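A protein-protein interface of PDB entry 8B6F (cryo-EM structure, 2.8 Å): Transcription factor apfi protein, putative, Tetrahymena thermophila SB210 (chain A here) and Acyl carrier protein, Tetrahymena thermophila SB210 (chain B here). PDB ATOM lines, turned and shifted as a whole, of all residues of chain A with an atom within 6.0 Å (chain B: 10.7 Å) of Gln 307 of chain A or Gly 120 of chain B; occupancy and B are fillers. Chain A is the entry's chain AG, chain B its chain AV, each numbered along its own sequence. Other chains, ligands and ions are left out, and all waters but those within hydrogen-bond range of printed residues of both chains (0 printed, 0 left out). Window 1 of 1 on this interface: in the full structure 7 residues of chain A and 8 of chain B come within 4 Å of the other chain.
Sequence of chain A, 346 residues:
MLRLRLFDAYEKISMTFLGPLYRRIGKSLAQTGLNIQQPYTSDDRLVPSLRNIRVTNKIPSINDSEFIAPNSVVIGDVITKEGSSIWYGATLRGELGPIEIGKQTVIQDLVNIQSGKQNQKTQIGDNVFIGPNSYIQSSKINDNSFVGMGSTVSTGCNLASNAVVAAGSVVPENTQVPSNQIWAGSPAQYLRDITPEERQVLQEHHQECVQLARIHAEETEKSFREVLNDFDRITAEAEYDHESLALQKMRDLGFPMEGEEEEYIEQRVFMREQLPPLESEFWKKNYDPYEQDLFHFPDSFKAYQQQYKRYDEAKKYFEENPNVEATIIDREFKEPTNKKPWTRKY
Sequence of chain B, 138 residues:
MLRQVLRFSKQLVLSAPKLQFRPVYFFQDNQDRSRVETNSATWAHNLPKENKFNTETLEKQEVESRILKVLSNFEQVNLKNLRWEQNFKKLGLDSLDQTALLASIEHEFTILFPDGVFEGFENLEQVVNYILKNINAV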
ATOM      1  N   LYS A 302     -16.800   8.727  23.111  1.00  0.00           N
ATOM      2  CA  LYS A 302     -16.570   9.597  24.260  1.00  0.00           C
ATOM      3  C   LYS A 302     -17.412  10.863  24.182  1.00  0.00           C
ATOM      4  O   LYS A 302     -17.711  11.473  25.214  1.00  0.00           O
ATOM      5  CB  LYS A 302     -15.088   9.957  24.361  1.00  0.00           C
ATOM      6  CG  LYS A 302     -14.193   8.810  24.793  1.00  0.00           C
ATOM      7  CD  LYS A 302     -12.746   9.261  24.904  1.00  0.00           C
ATOM      8  CE  LYS A 302     -11.866   8.164  25.476  1.00  0.00           C
ATOM      9  NZ  LYS A 302     -10.449   8.602  25.607  1.00  0.00           N
ATOM     10  N   ALA A 303     -17.794  11.277  22.974  1.00  0.00           N
ATOM     11  CA  ALA A 303     -18.640  12.457  22.834  1.00  0.00           C
ATOM     12  C   ALA A 303     -19.945  12.306  23.605  1.00  0.00           C
ATOM     13  O   ALA A 303     -20.550  13.310  23.997  1.00  0.00           O
ATOM     14  CB  ALA A 303     -18.927  12.725  21.358  1.00  0.00           C
ATOM     15  N   TYR A 304     -20.395  11.075  23.828  1.00  0.00           N
ATOM     16  CA  TYR A 304     -21.627  10.813  24.560  1.00  0.00           C
ATOM     17  C   TYR A 304     -21.415  10.691  26.064  1.00  0.00           C
ATOM     18  O   TYR A 304     -22.392  10.526  26.800  1.00  0.00           O
ATOM     19  CB  TYR A 304     -22.284   9.535  24.033  1.00  0.00           C
ATOM     20  CG  TYR A 304     -22.851   9.684  22.641  1.00  0.00           C
ATOM     21  CD1 TYR A 304     -24.154  10.117  22.446  1.00  0.00           C
ATOM     22  CD2 TYR A 304     -22.082   9.393  21.524  1.00  0.00           C
ATOM     23  CE1 TYR A 304     -24.678  10.257  21.178  1.00  0.00           C
ATOM     24  CE2 TYR A 304     -22.596   9.530  20.251  1.00  0.00           C
ATOM     25  CZ  TYR A 304     -23.894   9.962  20.085  1.00  0.00           C
ATOM     26  OH  TYR A 304     -24.415  10.099  18.820  1.00  0.00           O
ATOM     27  N   GLN A 305     -20.174  10.763  26.533  1.00  0.00           N
ATOM     28  CA  GLN A 305     -19.904  10.735  27.959  1.00  0.00           C
ATOM     29  C   GLN A 305     -20.355  12.043  28.606  1.00  0.00           C
ATOM     30  O   GLN A 305     -20.451  13.089  27.959  1.00  0.00           O
ATOM     31  CB  GLN A 305     -18.412  10.506  28.206  1.00  0.00           C
ATOM     32  CG  GLN A 305     -18.009  10.384  29.670  1.00  0.00           C
ATOM     33  CD  GLN A 305     -18.586   9.156  30.341  1.00  0.00           C
ATOM     34  OE1 GLN A 305     -19.218   9.247  31.392  1.00  0.00           O
ATOM     35  NE2 GLN A 305     -18.353   7.995  29.747  1.00  0.00           N
ATOM     36  N   GLN A 306     -20.643  11.971  29.902  1.00  0.00           N
ATOM     37  CA  GLN A 306     -21.008  13.167  30.648  1.00  0.00           C
ATOM     38  C   GLN A 306     -19.900  14.207  30.543  1.00  0.00           C
ATOM     39  O   GLN A 306     -18.712  13.885  30.618  1.00  0.00           O
ATOM     40  CB  GLN A 306     -21.276  12.815  32.110  1.00  0.00           C
ATOM     41  CG  GLN A 306     -21.656  14.002  32.983  1.00  0.00           C
ATOM     42  CD  GLN A 306     -21.937  13.600  34.417  1.00  0.00           C
ATOM     43  OE1 GLN A 306     -21.421  14.206  35.355  1.00  0.00           O
ATOM     44  NE2 GLN A 306     -22.766  12.579  34.595  1.00  0.00           N
ATOM     45  N   GLN A 307     -20.295  15.464  30.365  1.00  0.00           N
ATOM     46  CA  GLN A 307     -19.348  16.548  30.115  1.00  0.00           C
ATOM     47  C   GLN A 307     -18.762  17.014  31.440  1.00  0.00           C
ATOM     48  O   GLN A 307     -19.391  17.771  32.182  1.00  0.00           O
ATOM     49  CB  GLN A 307     -20.032  17.696  29.382  1.00  0.00           C
ATOM     50  CG  GLN A 307     -20.600  17.302  28.032  1.00  0.00           C
ATOM     51  CD  GLN A 307     -19.533  16.809  27.076  1.00  0.00           C
ATOM     52  OE1 GLN A 307     -18.383  17.244  27.136  1.00  0.00           O
ATOM     53  NE2 GLN A 307     -19.905  15.892  26.193  1.00  0.00           N
ATOM     54  N   TYR A 308     -17.542  16.566  31.733  1.00  0.00           N
ATOM     55  CA  TYR A 308     -16.864  16.971  32.957  1.00  0.00           C
ATOM     56  C   TYR A 308     -16.300  18.382  32.859  1.00  0.00           C
ATOM     57  O   TYR A 308     -16.127  19.048  33.885  1.00  0.00           O
ATOM     58  CB  TYR A 308     -15.742  15.986  33.280  1.00  0.00           C
ATOM     59  CG  TYR A 308     -16.171  14.540  33.218  1.00  0.00           C
ATOM     60  CD1 TYR A 308     -17.397  14.137  33.729  1.00  0.00           C
ATOM     61  CD2 TYR A 308     -15.358  13.583  32.631  1.00  0.00           C
ATOM     62  CE1 TYR A 308     -17.795  12.819  33.668  1.00  0.00           C
ATOM     63  CE2 TYR A 308     -15.746  12.262  32.566  1.00  0.00           C
ATOM     64  CZ  TYR A 308     -16.965  11.886  33.088  1.00  0.00           C
ATOM     65  OH  TYR A 308     -17.357  10.571  33.023  1.00  0.00           O
ATOM     66  N   LYS A 309     -16.012  18.852  31.645  1.00  0.00           N
ATOM     67  CA  LYS A 309     -15.511  20.211  31.481  1.00  0.00           C
ATOM     68  C   LYS A 309     -16.546  21.233  31.929  1.00  0.00           C
ATOM     69  O   LYS A 309     -16.198  22.270  32.504  1.00  0.00           O
ATOM     70  CB  LYS A 309     -15.103  20.451  30.030  1.00  0.00           C
ATOM     71  CG  LYS A 309     -13.936  19.588  29.581  1.00  0.00           C
ATOM     72  CD  LYS A 309     -13.474  19.950  28.180  1.00  0.00           C
ATOM     73  CE  LYS A 309     -12.329  19.058  27.728  1.00  0.00           C
ATOM     74  NZ  LYS A 309     -11.149  19.146  28.634  1.00  0.00           N
ATOM     75  N   ARG A 310     -17.825  20.959  31.676  1.00  0.00           N
ATOM     76  CA  ARG A 310     -18.872  21.858  32.149  1.00  0.00           C
ATOM     77  C   ARG A 310     -18.892  21.918  33.670  1.00  0.00           C
ATOM     78  O   ARG A 310     -19.067  22.994  34.252  1.00  0.00           O
ATOM     79  CB  ARG A 310     -20.230  21.412  31.607  1.00  0.00           C
ATOM     80  CG  ARG A 310     -20.362  21.535  30.094  1.00  0.00           C
ATOM     81  CD  ARG A 310     -20.145  22.967  29.623  1.00  0.00           C
ATOM     82  NE  ARG A 310     -20.423  23.129  28.201  1.00  0.00           N
ATOM     83  CZ  ARG A 310     -21.612  23.419  27.692  1.00  0.00           C
ATOM     84  NH1 ARG A 310     -22.678  23.569  28.463  1.00  0.00           N
ATOM     85  NH2 ARG A 310     -21.737  23.562  26.376  1.00  0.00           N
ATOM     86  N   TYR A 311     -18.719  20.773  34.334  1.00  0.00           N
ATOM     87  CA  TYR A 311     -18.659  20.780  35.791  1.00  0.00           C
ATOM     88  C   TYR A 311     -17.467  21.587  36.285  1.00  0.00           C
ATOM     89  O   TYR A 311     -17.585  22.355  37.246  1.00  0.00           O
ATOM     90  CB  TYR A 311     -18.591  19.348  36.321  1.00  0.00           C
ATOM     91  CG  TYR A 311     -19.902  18.607  36.237  1.00  0.00           C
ATOM     92  CD1 TYR A 311     -20.262  17.922  35.087  1.00  0.00           C
ATOM     93  CD2 TYR A 311     -20.780  18.591  37.312  1.00  0.00           C
ATOM     94  CE1 TYR A 311     -21.459  17.243  35.006  1.00  0.00           C
ATOM     95  CE2 TYR A 311     -21.980  17.915  37.242  1.00  0.00           C
ATOM     96  CZ  TYR A 311     -22.314  17.242  36.086  1.00  0.00           C
ATOM     97  OH  TYR A 311     -23.509  16.567  36.010  1.00  0.00           O
ATOM     98  N   ASP A 312     -16.305  21.422  35.650  1.00  0.00           N
ATOM     99  CA  ASP A 312     -15.131  22.186  36.060  1.00  0.00           C
ATOM    100  C   ASP A 312     -15.355  23.681  35.871  1.00  0.00           C
ATOM    101  O   ASP A 312     -14.988  24.485  36.736  1.00  0.00           O
ATOM    102  CB  ASP A 312     -13.904  21.726  35.273  1.00  0.00           C
ATOM    103  CG  ASP A 312     -13.517  20.295  35.585  1.00  0.00           C
ATOM    104  OD1 ASP A 312     -13.765  19.845  36.722  1.00  0.00           O
ATOM    105  OD2 ASP A 312     -12.965  19.618  34.694  1.00  0.00           O
ATOM    106  N   GLN B  86     -17.950  30.521  16.278  1.00  0.00           N
ATOM    107  CA  GLN B  86     -17.898  31.231  17.546  1.00  0.00           C
ATOM    108  C   GLN B  86     -18.825  30.581  18.567  1.00  0.00           C
ATOM    109  O   GLN B  86     -19.807  29.916  18.226  1.00  0.00           O
ATOM    110  CB  GLN B  86     -18.281  32.700  17.355  1.00  0.00           C
ATOM    111  CG  GLN B  86     -17.228  33.520  16.630  1.00  0.00           C
ATOM    112  CD  GLN B  86     -17.620  34.976  16.502  1.00  0.00           C
ATOM    113  OE1 GLN B  86     -18.668  35.396  16.991  1.00  0.00           O
ATOM    114  NE2 GLN B  86     -16.778  35.758  15.833  1.00  0.00           N
ATOM    115  N   ASN B  87     -18.498  30.784  19.837  1.00  0.00           N
ATOM    116  CA  ASN B  87     -19.282  30.212  20.918  1.00  0.00           C
ATOM    117  C   ASN B  87     -20.613  30.939  21.062  1.00  0.00           C
ATOM    118  O   ASN B  87     -20.788  32.074  20.612  1.00  0.00           O
ATOM    119  CB  ASN B  87     -18.516  30.285  22.238  1.00  0.00           C
ATOM    120  CG  ASN B  87     -17.205  29.536  22.193  1.00  0.00           C
ATOM    121  OD1 ASN B  87     -16.671  29.259  21.119  1.00  0.00           O
ATOM    122  ND2 ASN B  87     -16.676  29.201  23.363  1.00  0.00           N
ATOM    123  N   PHE B  88     -21.563  30.261  21.707  1.00  0.00           N
ATOM    124  CA  PHE B  88     -22.852  30.883  21.980  1.00  0.00           C
ATOM    125  C   PHE B  88     -22.686  32.145  22.814  1.00  0.00           C
ATOM    126  O   PHE B  88     -23.439  33.110  22.639  1.00  0.00           O
ATOM    127  CB  PHE B  88     -23.772  29.896  22.693  1.00  0.00           C
ATOM    128  CG  PHE B  88     -24.068  28.657  21.899  1.00  0.00           C
ATOM    129  CD1 PHE B  88     -24.934  28.701  20.820  1.00  0.00           C
ATOM    130  CD2 PHE B  88     -23.504  27.444  22.250  1.00  0.00           C
ATOM    131  CE1 PHE B  88     -25.217  27.561  20.096  1.00  0.00           C
ATOM    132  CE2 PHE B  88     -23.784  26.300  21.531  1.00  0.00           C
ATOM    133  CZ  PHE B  88     -24.642  26.359  20.451  1.00  0.00           C
ATOM    134  N   GLN B  98     -28.806  29.331  25.561  1.00  0.00           N
ATOM    135  CA  GLN B  98     -28.292  28.161  24.852  1.00  0.00           C
ATOM    136  C   GLN B  98     -29.248  26.981  24.958  1.00  0.00           C
ATOM    137  O   GLN B  98     -29.531  26.302  23.965  1.00  0.00           O
ATOM    138  CB  GLN B  98     -26.924  27.776  25.414  1.00  0.00           C
ATOM    139  CG  GLN B  98     -25.833  28.778  25.123  1.00  0.00           C
ATOM    140  CD  GLN B  98     -24.593  28.535  25.956  1.00  0.00           C
ATOM    141  OE1 GLN B  98     -24.397  27.446  26.494  1.00  0.00           O
ATOM    142  NE2 GLN B  98     -23.750  29.555  26.073  1.00  0.00           N
ATOM    143  N   THR B  99     -29.757  26.718  26.163  1.00  0.00           N
ATOM    144  CA  THR B  99     -30.696  25.617  26.341  1.00  0.00           C
ATOM    145  C   THR B  99     -31.964  25.847  25.534  1.00  0.00           C
ATOM    146  O   THR B  99     -32.489  24.921  24.907  1.00  0.00           O
ATOM    147  CB  THR B  99     -31.004  25.437  27.826  1.00  0.00           C
ATOM    148  OG1 THR B  99     -31.424  26.688  28.376  1.00  0.00           O
ATOM    149  CG2 THR B  99     -29.782  24.933  28.578  1.00  0.00           C
ATOM    150  N   LEU B 102     -31.151  25.251  21.802  1.00  0.00           N
ATOM    151  CA  LEU B 102     -31.003  23.836  21.483  1.00  0.00           C
ATOM    152  C   LEU B 102     -32.348  23.123  21.507  1.00  0.00           C
ATOM    153  O   LEU B 102     -32.613  22.257  20.666  1.00  0.00           O
ATOM    154  CB  LEU B 102     -30.019  23.182  22.451  1.00  0.00           C
ATOM    155  CG  LEU B 102     -28.569  23.672  22.362  1.00  0.00           C
ATOM    156  CD1 LEU B 102     -27.700  22.963  23.385  1.00  0.00           C
ATOM    157  CD2 LEU B 102     -27.998  23.483  20.964  1.00  0.00           C
ATOM    158  N   GLU B 106     -34.130  21.220  18.419  1.00  0.00           N
ATOM    159  CA  GLU B 106     -34.704  19.884  18.540  1.00  0.00           C
ATOM    160  C   GLU B 106     -36.141  19.859  18.038  1.00  0.00           C
ATOM    161  O   GLU B 106     -36.541  18.938  17.319  1.00  0.00           O
ATOM    162  CB  GLU B 106     -34.648  19.415  19.994  1.00  0.00           C
ATOM    163  CG  GLU B 106     -33.259  19.058  20.486  1.00  0.00           C
ATOM    164  CD  GLU B 106     -33.267  18.556  21.916  1.00  0.00           C
ATOM    165  OE1 GLU B 106     -34.358  18.491  22.516  1.00  0.00           O
ATOM    166  OE2 GLU B 106     -32.185  18.226  22.441  1.00  0.00           O
ATOM    167  N   PHE B 113     -31.564  15.404  21.456  1.00  0.00           N
ATOM    168  CA  PHE B 113     -30.138  15.303  21.739  1.00  0.00           C
ATOM    169  C   PHE B 113     -29.918  14.557  23.050  1.00  0.00           C
ATOM    170  O   PHE B 113     -30.447  14.980  24.084  1.00  0.00           O
ATOM    171  CB  PHE B 113     -29.513  16.690  21.833  1.00  0.00           C
ATOM    172  CG  PHE B 113     -29.537  17.464  20.545  1.00  0.00           C
ATOM    173  CD1 PHE B 113     -29.232  16.852  19.341  1.00  0.00           C
ATOM    174  CD2 PHE B 113     -29.860  18.811  20.544  1.00  0.00           C
ATOM    175  CE1 PHE B 113     -29.252  17.569  18.161  1.00  0.00           C
ATOM    176  CE2 PHE B 113     -29.882  19.533  19.368  1.00  0.00           C
ATOM    177  CZ  PHE B 113     -29.578  18.911  18.176  1.00  0.00           C
ATOM    178  N   PRO B 114     -29.160  13.453  23.061  1.00  0.00           N
ATOM    179  CA  PRO B 114     -28.754  12.860  24.341  1.00  0.00           C
ATOM    180  C   PRO B 114     -28.164  13.897  25.282  1.00  0.00           C
ATOM    181  O   PRO B 114     -27.737  14.968  24.840  1.00  0.00           O
ATOM    182  CB  PRO B 114     -27.709  11.815  23.933  1.00  0.00           C
ATOM    183  CG  PRO B 114     -27.979  11.506  22.501  1.00  0.00           C
ATOM    184  CD  PRO B 114     -28.920  12.534  21.934  1.00  0.00           C
ATOM    185  N   ASP B 115     -28.133  13.594  26.580  1.00  0.00           N
ATOM    186  CA  ASP B 115     -27.634  14.567  27.548  1.00  0.00           C
ATOM    187  C   ASP B 115     -26.179  14.921  27.276  1.00  0.00           C
ATOM    188  O   ASP B 115     -25.795  16.093  27.352  1.00  0.00           O
ATOM    189  CB  ASP B 115     -27.797  14.028  28.968  1.00  0.00           C
ATOM    190  CG  ASP B 115     -29.248  13.836  29.355  1.00  0.00           C
ATOM    191  OD1 ASP B 115     -30.101  14.599  28.856  1.00  0.00           O
ATOM    192  OD2 ASP B 115     -29.538  12.926  30.158  1.00  0.00           O
ATOM    193  N   GLY B 116     -25.351  13.922  26.967  1.00  0.00           N
ATOM    194  CA  GLY B 116     -23.937  14.191  26.761  1.00  0.00           C
ATOM    195  C   GLY B 116     -23.688  15.158  25.620  1.00  0.00           C
ATOM    196  O   GLY B 116     -22.939  16.126  25.761  1.00  0.00           O
ATOM    197  N   VAL B 117     -24.306  14.901  24.465  1.00  0.00           N
ATOM    198  CA  VAL B 117     -24.106  15.776  23.314  1.00  0.00           C
ATOM    199  C   VAL B 117     -24.762  17.132  23.548  1.00  0.00           C
ATOM    200  O   VAL B 117     -24.203  18.173  23.188  1.00  0.00           O
ATOM    201  CB  VAL B 117     -24.628  15.103  22.030  1.00  0.00           C
ATOM    202  CG1 VAL B 117     -23.926  13.774  21.804  1.00  0.00           C
ATOM    203  CG2 VAL B 117     -26.132  14.910  22.084  1.00  0.00           C
ATOM    204  N   PHE B 118     -25.946  17.144  24.162  1.00  0.00           N
ATOM    205  CA  PHE B 118     -26.631  18.405  24.434  1.00  0.00           C
ATOM    206  C   PHE B 118     -25.757  19.328  25.272  1.00  0.00           C
ATOM    207  O   PHE B 118     -25.643  20.526  24.986  1.00  0.00           O
ATOM    208  CB  PHE B 118     -27.959  18.133  25.143  1.00  0.00           C
ATOM    209  CG  PHE B 118     -28.859  19.334  25.240  1.00  0.00           C
ATOM    210  CD1 PHE B 118     -28.569  20.368  26.114  1.00  0.00           C
ATOM    211  CD2 PHE B 118     -30.010  19.415  24.478  1.00  0.00           C
ATOM    212  CE1 PHE B 118     -29.399  21.466  26.209  1.00  0.00           C
ATOM    213  CE2 PHE B 118     -30.843  20.512  24.570  1.00  0.00           C
ATOM    214  CZ  PHE B 118     -30.536  21.537  25.435  1.00  0.00           C
ATOM    215  N   GLU B 119     -25.133  18.788  26.315  1.00  0.00           N
ATOM    216  CA  GLU B 119     -24.249  19.577  27.159  1.00  0.00           C
ATOM    217  C   GLU B 119     -22.891  19.822  26.518  1.00  0.00           C
ATOM    218  O   GLU B 119     -22.203  20.771  26.906  1.00  0.00           O
ATOM    219  CB  GLU B 119     -24.059  18.884  28.510  1.00  0.00           C
ATOM    220  CG  GLU B 119     -25.357  18.671  29.276  1.00  0.00           C
ATOM    221  CD  GLU B 119     -25.148  17.938  30.587  1.00  0.00           C
ATOM    222  OE1 GLU B 119     -23.980  17.755  30.988  1.00  0.00           O
ATOM    223  OE2 GLU B 119     -26.153  17.542  31.214  1.00  0.00           O
ATOM    224  N   GLY B 120     -22.491  18.995  25.550  1.00  0.00           N
ATOM    225  CA  GLY B 120     -21.203  19.180  24.907  1.00  0.00           C
ATOM    226  C   GLY B 120     -21.189  20.186  23.780  1.00  0.00           C
ATOM    227  O   GLY B 120     -20.116  20.687  23.432  1.00  0.00           O
ATOM    228  N   PHE B 121     -22.346  20.488  23.192  1.00  0.00           N
ATOM    229  CA  PHE B 121     -22.400  21.480  22.126  1.00  0.00           C
ATOM    230  C   PHE B 121     -21.843  22.811  22.615  1.00  0.00           C
ATOM    231  O   PHE B 121     -22.204  23.290  23.694  1.00  0.00           O
ATOM    232  CB  PHE B 121     -23.837  21.663  21.637  1.00  0.00           C
ATOM    233  CG  PHE B 121     -24.357  20.517  20.814  1.00  0.00           C
ATOM    234  CD1 PHE B 121     -23.543  19.860  19.906  1.00  0.00           C
ATOM    235  CD2 PHE B 121     -25.670  20.104  20.944  1.00  0.00           C
ATOM    236  CE1 PHE B 121     -24.027  18.812  19.154  1.00  0.00           C
ATOM    237  CE2 PHE B 121     -26.160  19.059  20.194  1.00  0.00           C
ATOM    238  CZ  PHE B 121     -25.337  18.412  19.298  1.00  0.00           C
ATOM    239  N   GLU B 122     -20.963  23.410  21.812  1.00  0.00           N
ATOM    240  CA  GLU B 122     -20.355  24.690  22.139  1.00  0.00           C
ATOM    241  C   GLU B 122     -20.569  25.762  21.085  1.00  0.00           C
ATOM    242  O   GLU B 122     -20.348  26.940  21.381  1.00  0.00           O
ATOM    243  CB  GLU B 122     -18.843  24.524  22.361  1.00  0.00           C
ATOM    244  CG  GLU B 122     -18.492  23.636  23.538  1.00  0.00           C
ATOM    245  CD  GLU B 122     -16.998  23.464  23.706  1.00  0.00           C
ATOM    246  OE1 GLU B 122     -16.238  24.089  22.936  1.00  0.00           O
ATOM    247  OE2 GLU B 122     -16.581  22.704  24.605  1.00  0.00           O
ATOM    248  N   ASN B 123     -20.986  25.400  19.876  1.00  0.00           N
ATOM    249  CA  ASN B 123     -21.234  26.371  18.821  1.00  0.00           C
ATOM    250  C   ASN B 123     -22.196  25.746  17.819  1.00  0.00           C
ATOM    251  O   ASN B 123     -22.561  24.572  17.927  1.00  0.00           O
ATOM    252  CB  ASN B 123     -19.925  26.815  18.162  1.00  0.00           C
ATOM    253  CG  ASN B 123     -19.090  25.648  17.681  1.00  0.00           C
ATOM    254  OD1 ASN B 123     -19.619  24.638  17.223  1.00  0.00           O
ATOM    255  ND2 ASN B 123     -17.774  25.779  17.791  1.00  0.00           N
ATOM    256  N   LEU B 124     -22.610  26.549  16.837  1.00  0.00           N
ATOM    257  CA  LEU B 124     -23.599  26.083  15.870  1.00  0.00           C
ATOM    258  C   LEU B 124     -23.009  25.081  14.888  1.00  0.00           C
ATOM    259  O   LEU B 124     -23.739  24.239  14.356  1.00  0.00           O
ATOM    260  CB  LEU B 124     -24.196  27.270  15.117  1.00  0.00           C
ATOM    261  CG  LEU B 124     -24.999  28.262  15.960  1.00  0.00           C
ATOM    262  CD1 LEU B 124     -25.362  29.483  15.137  1.00  0.00           C
ATOM    263  CD2 LEU B 124     -26.252  27.608  16.520  1.00  0.00           C
ATOM    264  N   GLU B 125     -21.700  25.139  14.644  1.00  0.00           N
ATOM    265  CA  GLU B 125     -21.087  24.205  13.705  1.00  0.00           C
ATOM    266  C   GLU B 125     -21.209  22.770  14.202  1.00  0.00           C
ATOM    267  O   GLU B 125     -21.487  21.856  13.418  1.00  0.00           O
ATOM    268  CB  GLU B 125     -19.620  24.571  13.483  1.00  0.00           C
ATOM    269  CG  GLU B 125     -18.933  23.720  12.430  1.00  0.00           C
ATOM    270  CD  GLU B 125     -17.503  24.152  12.177  1.00  0.00           C
ATOM    271  OE1 GLU B 125     -17.087  25.184  12.742  1.00  0.00           O
ATOM    272  OE2 GLU B 125     -16.796  23.456  11.419  1.00  0.00           O
ATOM    273  N   GLN B 126     -21.004  22.553  15.501  1.00  0.00           N
ATOM    274  CA  GLN B 126     -21.146  21.213  16.055  1.00  0.00           C
ATOM    275  C   GLN B 126     -22.576  20.710  15.909  1.00  0.00           C
ATOM    276  O   GLN B 126     -22.801  19.540  15.583  1.00  0.00           O
ATOM    277  CB  GLN B 126     -20.719  21.201  17.522  1.00  0.00           C
ATOM    278  CG  GLN B 126     -19.246  21.505  17.731  1.00  0.00           C
ATOM    279  CD  GLN B 126     -18.888  21.653  19.191  1.00  0.00           C
ATOM    280  OE1 GLN B 126     -19.720  21.445  20.070  1.00  0.00           O
ATOM    281  NE2 GLN B 126     -17.639  22.010  19.459  1.00  0.00           N
ATOM    282  N   VAL B 127     -23.558  21.580  16.153  1.00  0.00           N
ATOM    283  CA  VAL B 127     -24.954  21.189  15.986  1.00  0.00           C
ATOM    284  C   VAL B 127     -25.229  20.826  14.533  1.00  0.00           C
ATOM    285  O   VAL B 127     -25.917  19.840  14.243  1.00  0.00           O
ATOM    286  CB  VAL B 127     -25.887  22.313  16.473  1.00  0.00           C
ATOM    287  CG1 VAL B 127     -27.343  21.910  16.305  1.00  0.00           C
ATOM    288  CG2 VAL B 127     -25.595  22.657  17.922  1.00  0.00           C
ATOM    289  N   TYR B 130     -23.724  17.408  13.813  1.00  0.00           N
ATOM    290  CA  TYR B 130     -24.493  16.340  14.441  1.00  0.00           C
ATOM    291  C   TYR B 130     -25.788  16.075  13.684  1.00  0.00           C
ATOM    292  O   TYR B 130     -26.156  14.919  13.456  1.00  0.00           O
ATOM    293  CB  TYR B 130     -24.789  16.696  15.898  1.00  0.00           C
ATOM    294  CG  TYR B 130     -25.550  15.624  16.640  1.00  0.00           C
ATOM    295  CD1 TYR B 130     -26.939  15.600  16.640  1.00  0.00           C
ATOM    296  CD2 TYR B 130     -24.878  14.631  17.336  1.00  0.00           C
ATOM    297  CE1 TYR B 130     -27.636  14.620  17.314  1.00  0.00           C
ATOM    298  CE2 TYR B 130     -25.564  13.645  18.012  1.00  0.00           C
ATOM    299  CZ  TYR B 130     -26.941  13.645  17.999  1.00  0.00           C
ATOM    300  OH  TYR B 130     -27.624  12.663  18.675  1.00  0.00           O
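NH2 of Arg 310 of chain A is in hydrogen-bond range of O of Phe 121 of chain B, 2.7 Å away. NH2 of Arg 310 of chain A lies close to O of Glu 119 of chain B (2.9 Å). The side-chain amide nitrogen (NE2) of Gln 307 of chain A is in hydrogen-bond range of the backbone carbonyl oxygen (O) of Gly 116 of chain B, at 3.1 Å.
The backbone carbonyl oxygen (O) of Ala 303 of chain A is in hydrogen-bond range of the side-chain amide nitrogen (NE2) of Gln 307 of chain A, at 3.5 Å. The side-chain amide oxygen (OE1) of Gln 126 of chain B lies close to the backbone carbonyl oxygen (O) of Gly 120 of chain B, 3.5 Å away. The backbone carbonyl oxygen (O) of Gln 305 of chain A lies within hydrogen-bond range of the side-chain amide nitrogen (NE2) of Gln 307 of chain A, at 3.4 Å. The side-chain amide oxygen of Gln 305 of chain A sits at hydrogen-bond distance from the side-chain hydroxyl of Tyr 308 of chain A, at 2.8 Å.
O of Ala 303 of chain A touches C of Gly 116 of chain B, at 3.99 Å. Pro 114 of chain B touches Tyr 304 of chain A. O of Tyr 304 of chain A touches CA of Gly 116 of chain B, 3.98 Å away. CG1 of Val 117 of chain B touches CE1 of Tyr 304 of chain A, at 3.7 Å. Tyr 304 of chain A touches Tyr 130 of chain B (OH to CE2, 3.8 Å). O of Gln 305 of chain A touches CA of Gly 116 of chain B, at 3.8 Å. Gln 307 of chain A touches Glu 119 of chain B (CG to C, 3.7 Å). Gly 120 of chain B touches Gln 307 of chain A (N to CG, 3.5 Å).
Printed residues of chain B within 4 Å of Gln 307 of chain A: Gly 116, Glu 119 and Gly 120. Gly 120 of chain B touches just one residue of chain A: Gln 307 (3.5 Å). No residue of chain B comes within 4 Å of Gln 306 of chain A. Of chain B, only Glu 119 (2.8 Å) and Phe 121 (2.7 Å) come within 4 Å of Arg 310 of chain A. Of the printed residues of chain A, Glu 119 of chain B touches Gln 307 and Arg 310. Printed residues of chain B within 4 Å of Gln 305 of chain A: Gly 116. Gln 86 of chain B touches none of the printed residues of chain A. The nearest printed residue of chain A that does not touch Tyr 130 of chain B is Ala 303 of chain A (7.4 Å).
Of the 23 printed residues of chain B, 7 touch a printed residue of chain A. Printed residues of chain B that touch a printed residue of chain A: Pro 114, Gly 116, Val 117, Glu 119, Gly 120, Phe 121 and Tyr 130. Of the 11 printed residues of chain A, 5 touch a printed residue of chain B. Hydrophobic or aromatic side chains of chain A that line the printed part of chain B: Tyr 304. Among the printed residues, no Asp or Glu carboxylate lies within 4 Å of a Lys or Arg side-chain nitrogen of the other chain.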
